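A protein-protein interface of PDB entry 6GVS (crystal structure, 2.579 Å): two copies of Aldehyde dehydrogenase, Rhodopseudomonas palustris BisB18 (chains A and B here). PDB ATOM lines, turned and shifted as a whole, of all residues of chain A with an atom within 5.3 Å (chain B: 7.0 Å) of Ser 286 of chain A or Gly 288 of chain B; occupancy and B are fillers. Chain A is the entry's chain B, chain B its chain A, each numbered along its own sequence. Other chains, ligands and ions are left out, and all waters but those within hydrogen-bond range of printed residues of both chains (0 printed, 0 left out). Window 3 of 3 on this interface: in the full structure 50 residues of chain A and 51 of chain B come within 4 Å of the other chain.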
ATOM      1  N   LYS A 282     -25.933  37.067  27.250  1.00  0.00           N
ATOM      2  CA  LYS A 282     -26.211  35.714  27.721  1.00  0.00           C
ATOM      3  C   LYS A 282     -27.691  35.382  27.576  1.00  0.00           C
ATOM      4  O   LYS A 282     -28.046  34.276  27.152  1.00  0.00           O
ATOM      5  CB  LYS A 282     -25.764  35.560  29.173  1.00  0.00           C
ATOM      6  CG  LYS A 282     -25.983  34.169  29.755  1.00  0.00           C
ATOM      7  CD  LYS A 282     -25.561  34.119  31.218  1.00  0.00           C
ATOM      8  CE  LYS A 282     -26.009  32.831  31.889  1.00  0.00           C
ATOM      9  NZ  LYS A 282     -25.815  32.883  33.366  1.00  0.00           N
ATOM     10  N   ALA A 283     -28.566  36.330  27.923  1.00  0.00           N
ATOM     11  CA  ALA A 283     -29.998  36.121  27.746  1.00  0.00           C
ATOM     12  C   ALA A 283     -30.323  35.782  26.298  1.00  0.00           C
ATOM     13  O   ALA A 283     -30.961  34.763  26.012  1.00  0.00           O
ATOM     14  CB  ALA A 283     -30.767  37.367  28.188  1.00  0.00           C
ATOM     15  N   VAL A 284     -29.880  36.627  25.367  1.00  0.00           N
ATOM     16  CA  VAL A 284     -30.184  36.422  23.955  1.00  0.00           C
ATOM     17  C   VAL A 284     -29.650  35.086  23.456  1.00  0.00           C
ATOM     18  O   VAL A 284     -30.225  34.485  22.541  1.00  0.00           O
ATOM     19  CB  VAL A 284     -29.620  37.602  23.138  1.00  0.00           C
ATOM     20  CG1 VAL A 284     -29.429  37.209  21.690  1.00  0.00           C
ATOM     21  CG2 VAL A 284     -30.542  38.814  23.255  1.00  0.00           C
ATOM     22  N   LEU A 285     -28.554  34.598  24.034  1.00  0.00           N
ATOM     23  CA  LEU A 285     -27.996  33.311  23.636  1.00  0.00           C
ATOM     24  C   LEU A 285     -28.679  32.132  24.320  1.00  0.00           C
ATOM     25  O   LEU A 285     -28.263  30.985  24.106  1.00  0.00           O
ATOM     26  CB  LEU A 285     -26.495  33.280  23.929  1.00  0.00           C
ATOM     27  CG  LEU A 285     -25.624  34.100  22.977  1.00  0.00           C
ATOM     28  CD1 LEU A 285     -24.252  34.335  23.582  1.00  0.00           C
ATOM     29  CD2 LEU A 285     -25.504  33.406  21.626  1.00  0.00           C
ATOM     30  N   SER A 286     -29.710  32.384  25.129  1.00  0.00           N
ATOM     31  CA  SER A 286     -30.466  31.336  25.802  1.00  0.00           C
ATOM     32  C   SER A 286     -31.897  31.239  25.283  1.00  0.00           C
ATOM     33  O   SER A 286     -32.777  30.737  25.988  1.00  0.00           O
ATOM     34  CB  SER A 286     -30.477  31.582  27.312  1.00  0.00           C
ATOM     35  OG  SER A 286     -29.168  31.794  27.806  1.00  0.00           O
ATOM     36  N   THR A 287     -32.143  31.704  24.060  1.00  0.00           N
ATOM     37  CA  THR A 287     -33.492  31.814  23.524  1.00  0.00           C
ATOM     38  C   THR A 287     -33.828  30.735  22.505  1.00  0.00           C
ATOM     39  O   THR A 287     -34.915  30.772  21.920  1.00  0.00           O
ATOM     40  CB  THR A 287     -33.681  33.187  22.871  1.00  0.00           C
ATOM     41  OG1 THR A 287     -32.880  33.259  21.682  1.00  0.00           O
ATOM     42  CG2 THR A 287     -33.275  34.296  23.831  1.00  0.00           C
ATOM     43  N   GLY A 288     -32.929  29.784  22.271  1.00  0.00           N
ATOM     44  CA  GLY A 288     -33.159  28.798  21.238  1.00  0.00           C
ATOM     45  C   GLY A 288     -33.149  29.344  19.831  1.00  0.00           C
ATOM     46  O   GLY A 288     -33.609  28.663  18.913  1.00  0.00           O
ATOM     47  N   MET B 264     -22.678  21.046  27.339  1.00  0.00           N
ATOM     48  CA  MET B 264     -23.417  22.260  27.018  1.00  0.00           C
ATOM     49  C   MET B 264     -23.422  23.254  28.173  1.00  0.00           C
ATOM     50  O   MET B 264     -23.614  24.453  27.943  1.00  0.00           O
ATOM     51  CB  MET B 264     -24.865  21.920  26.639  1.00  0.00           C
ATOM     52  CG  MET B 264     -25.007  20.961  25.462  1.00  0.00           C
ATOM     53  SD  MET B 264     -26.701  20.706  24.860  1.00  0.00           S
ATOM     54  CE  MET B 264     -27.683  21.373  26.202  1.00  0.00           C
ATOM     55  N   LEU B 272     -20.534  25.654  20.776  1.00  0.00           N
ATOM     56  CA  LEU B 272     -21.147  24.357  20.530  1.00  0.00           C
ATOM     57  C   LEU B 272     -21.383  24.183  19.037  1.00  0.00           C
ATOM     58  O   LEU B 272     -21.753  25.135  18.342  1.00  0.00           O
ATOM     59  CB  LEU B 272     -22.471  24.223  21.284  1.00  0.00           C
ATOM     60  CG  LEU B 272     -22.360  24.189  22.809  1.00  0.00           C
ATOM     61  CD1 LEU B 272     -23.733  24.256  23.451  1.00  0.00           C
ATOM     62  CD2 LEU B 272     -21.615  22.943  23.268  1.00  0.00           C
ATOM     63  N   ALA B 283     -31.668  22.899  21.588  1.00  0.00           N
ATOM     64  CA  ALA B 283     -31.078  22.767  22.916  1.00  0.00           C
ATOM     65  C   ALA B 283     -29.793  23.577  23.034  1.00  0.00           C
ATOM     66  O   ALA B 283     -29.596  24.309  24.010  1.00  0.00           O
ATOM     67  CB  ALA B 283     -30.815  21.293  23.226  1.00  0.00           C
ATOM     68  N   VAL B 284     -28.901  23.456  22.044  1.00  0.00           N
ATOM     69  CA  VAL B 284     -27.616  24.147  22.115  1.00  0.00           C
ATOM     70  C   VAL B 284     -27.795  25.650  21.946  1.00  0.00           C
ATOM     71  O   VAL B 284     -26.992  26.438  22.462  1.00  0.00           O
ATOM     72  CB  VAL B 284     -26.639  23.581  21.066  1.00  0.00           C
ATOM     73  CG1 VAL B 284     -26.371  22.105  21.339  1.00  0.00           C
ATOM     74  CG2 VAL B 284     -27.183  23.778  19.657  1.00  0.00           C
ATOM     75  N   LEU B 285     -28.837  26.075  21.231  1.00  0.00           N
ATOM     76  CA  LEU B 285     -29.160  27.491  21.104  1.00  0.00           C
ATOM     77  C   LEU B 285     -29.875  28.043  22.335  1.00  0.00           C
ATOM     78  O   LEU B 285     -30.360  29.179  22.299  1.00  0.00           O
ATOM     79  CB  LEU B 285     -30.020  27.726  19.861  1.00  0.00           C
ATOM     80  CG  LEU B 285     -29.351  27.461  18.513  1.00  0.00           C
ATOM     81  CD1 LEU B 285     -30.374  27.538  17.393  1.00  0.00           C
ATOM     82  CD2 LEU B 285     -28.220  28.440  18.252  1.00  0.00           C
ATOM     83  N   SER B 286     -29.946  27.265  23.417  1.00  0.00           N
ATOM     84  CA  SER B 286     -30.586  27.690  24.657  1.00  0.00           C
ATOM     85  C   SER B 286     -29.614  27.647  25.829  1.00  0.00           C
ATOM     86  O   SER B 286     -30.044  27.656  26.987  1.00  0.00           O
ATOM     87  CB  SER B 286     -31.806  26.816  24.958  1.00  0.00           C
ATOM     88  OG  SER B 286     -32.628  26.656  23.813  1.00  0.00           O
ATOM     89  N   THR B 287     -28.310  27.603  25.546  1.00  0.00           N
ATOM     90  CA  THR B 287     -27.288  27.409  26.562  1.00  0.00           C
ATOM     91  C   THR B 287     -26.580  28.692  26.967  1.00  0.00           C
ATOM     92  O   THR B 287     -25.805  28.675  27.928  1.00  0.00           O
ATOM     93  CB  THR B 287     -26.228  26.416  26.063  1.00  0.00           C
ATOM     94  OG1 THR B 287     -25.620  26.931  24.868  1.00  0.00           O
ATOM     95  CG2 THR B 287     -26.849  25.059  25.777  1.00  0.00           C
ATOM     96  N   GLY B 288     -26.809  29.791  26.258  1.00  0.00           N
ATOM     97  CA  GLY B 288     -26.036  30.992  26.494  1.00  0.00           C
ATOM     98  C   GLY B 288     -24.669  30.985  25.858  1.00  0.00           C
ATOM     99  O   GLY B 288     -23.815  31.790  26.242  1.00  0.00           O
ATOM    100  N   LYS B 289     -24.433  30.099  24.894  1.00  0.00           N
ATOM    101  CA  LYS B 289     -23.156  30.003  24.206  1.00  0.00           C
ATOM    102  C   LYS B 289     -23.354  30.178  22.705  1.00  0.00           C
ATOM    103  O   LYS B 289     -24.417  29.867  22.161  1.00  0.00           O
ATOM    104  CB  LYS B 289     -22.477  28.648  24.471  1.00  0.00           C
ATOM    105  CG  LYS B 289     -22.296  28.300  25.941  1.00  0.00           C
ATOM    106  CD  LYS B 289     -21.559  26.973  26.105  1.00  0.00           C
ATOM    107  CE  LYS B 289     -21.478  26.538  27.566  1.00  0.00           C
ATOM    108  NZ  LYS B 289     -20.620  27.435  28.387  1.00  0.00           N
ATOM    109  N   LYS B 290     -22.321  30.693  22.042  1.00  0.00           N
ATOM    110  CA  LYS B 290     -22.258  30.631  20.589  1.00  0.00           C
ATOM    111  C   LYS B 290     -22.449  29.188  20.143  1.00  0.00           C
ATOM    112  O   LYS B 290     -21.809  28.275  20.671  1.00  0.00           O
ATOM    113  CB  LYS B 290     -20.912  31.172  20.105  1.00  0.00           C
ATOM    114  CG  LYS B 290     -20.620  30.964  18.625  1.00  0.00           C
ATOM    115  CD  LYS B 290     -21.541  31.783  17.739  1.00  0.00           C
ATOM    116  CE  LYS B 290     -21.071  31.750  16.291  1.00  0.00           C
ATOM    117  NZ  LYS B 290     -22.016  32.442  15.374  1.00  0.00           N
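The backbone carbonyl oxygen (O) of Leu 285 of chain B is in hydrogen-bond range of the backbone NH (N) of Gly 288 of chain A (2.6 Å).
The backbone NH (N) of Gly 288 of chain B lies within hydrogen-bond range of the backbone carbonyl oxygen (O) of Leu 285 of chain A, at 2.9 Å.
N of Gly 288 of chain B sits at hydrogen-bond distance from OG of Ser 286 of chain A (3.5 Å).
The backbone carbonyl oxygen of Leu 285 of chain A sits close to the backbone carbonyl oxygen of Leu 285 of chain B (3.3 Å).
The backbone carbonyl oxygen of Val 284 of chain B sits at hydrogen-bond distance from the side-chain hydroxyl of Thr 287 of chain B (2.8 Å).
The side-chain hydroxyl (OG1) of Thr 287 of chain B lies close to the backbone NH (N) of Lys 289 of chain B (3.4 Å).
OG of Ser 286 of chain A sits at hydrogen-bond distance from O of Lys 282 of chain A (2.8 Å).
OG1 of Thr 287 of chain A sits at hydrogen-bond distance from O of Val 284 of chain A (3.0 Å).
CA of Gly 288 of chain B touches O of Lys 282 of chain A (3.9 Å).
O of Leu 285 of chain A touches C of Ser 286 of chain B, 3.99 Å away.
O of Leu 285 of chain A touches N of Thr 287 of chain B (3.7 Å).
Leu 285 of chain A touches Lys 289 of chain B.
C of Ser 286 of chain A touches O of Leu 285 of chain B, at 3.9 Å.
Ser 286 of chain B touches Ser 286 of chain A (C to CA, 3.8 Å).
Thr 287 of chain A touches Leu 285 of chain B.
Gly 288 of chain A touches Ser 286 of chain B.
Of chain B, only Leu 285, Ser 286 and Gly 288 come within 4 Å of Ser 286 of chain A.
Of chain A, only Lys 282, Leu 285 and Ser 286 come within 4 Å of Gly 288 of chain B.
Of the printed residues of chain A, Thr 287 of chain B touches Leu 285 (3.7 Å).
Printed residues of chain A within 4 Å of Lys 289 of chain B: Leu 285 (3.7 Å).
Of the printed residues of chain B, Leu 285 of chain A touches Leu 285, Ser 286, Thr 287, Gly 288 and Lys 289.
Printed residues of chain B within 4 Å of Thr 287 of chain A: Leu 285 (3.6 Å).
Lys 290 of chain B touches none of the printed residues of chain A.
The nearest printed residue of chain A that does not touch Gly 288 of chain B is Ala 283 of chain A (6.1 Å).
Printed residues of chain A that touch a printed residue of chain B: Lys 282, Leu 285, Ser 286, Thr 287 and Gly 288.
Along chain A the printed residues that touch a printed residue of chain B span positions 282 to 288.
Of the 10 printed residues of chain B, 5 touch a printed residue of chain A.
Hydrophobic or aromatic side chains of chain B that line the printed part of chain A: Leu 285.
Among the printed residues, no Asp or Glu carboxylate lies within 4 Å of a Lys or Arg side-chain nitrogen of the other chain.
Leu 285 of chain B touches its own counterpart, Leu 285 of chain A.
Leu 285 of chain A touches Ser 286 of chain B, and with the chains exchanged Ser 286 of chain A touches Leu 285 of chain B.
Leu 285 of chain A touches Thr 287 of chain B, and with the chains exchanged Thr 287 of chain A touches Leu 285 of chain B.
Leu 285 of chain A touches Gly 288 of chain B, and with the chains exchanged Gly 288 of chain A touches Leu 285 of chain B.
Positions printed for both chains: 283, 284, 285, 286, 287 and 288.
Of the 12 pairs that touch across the chains among the printed residues, 10 have their exchanged pair printed and touching as well.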
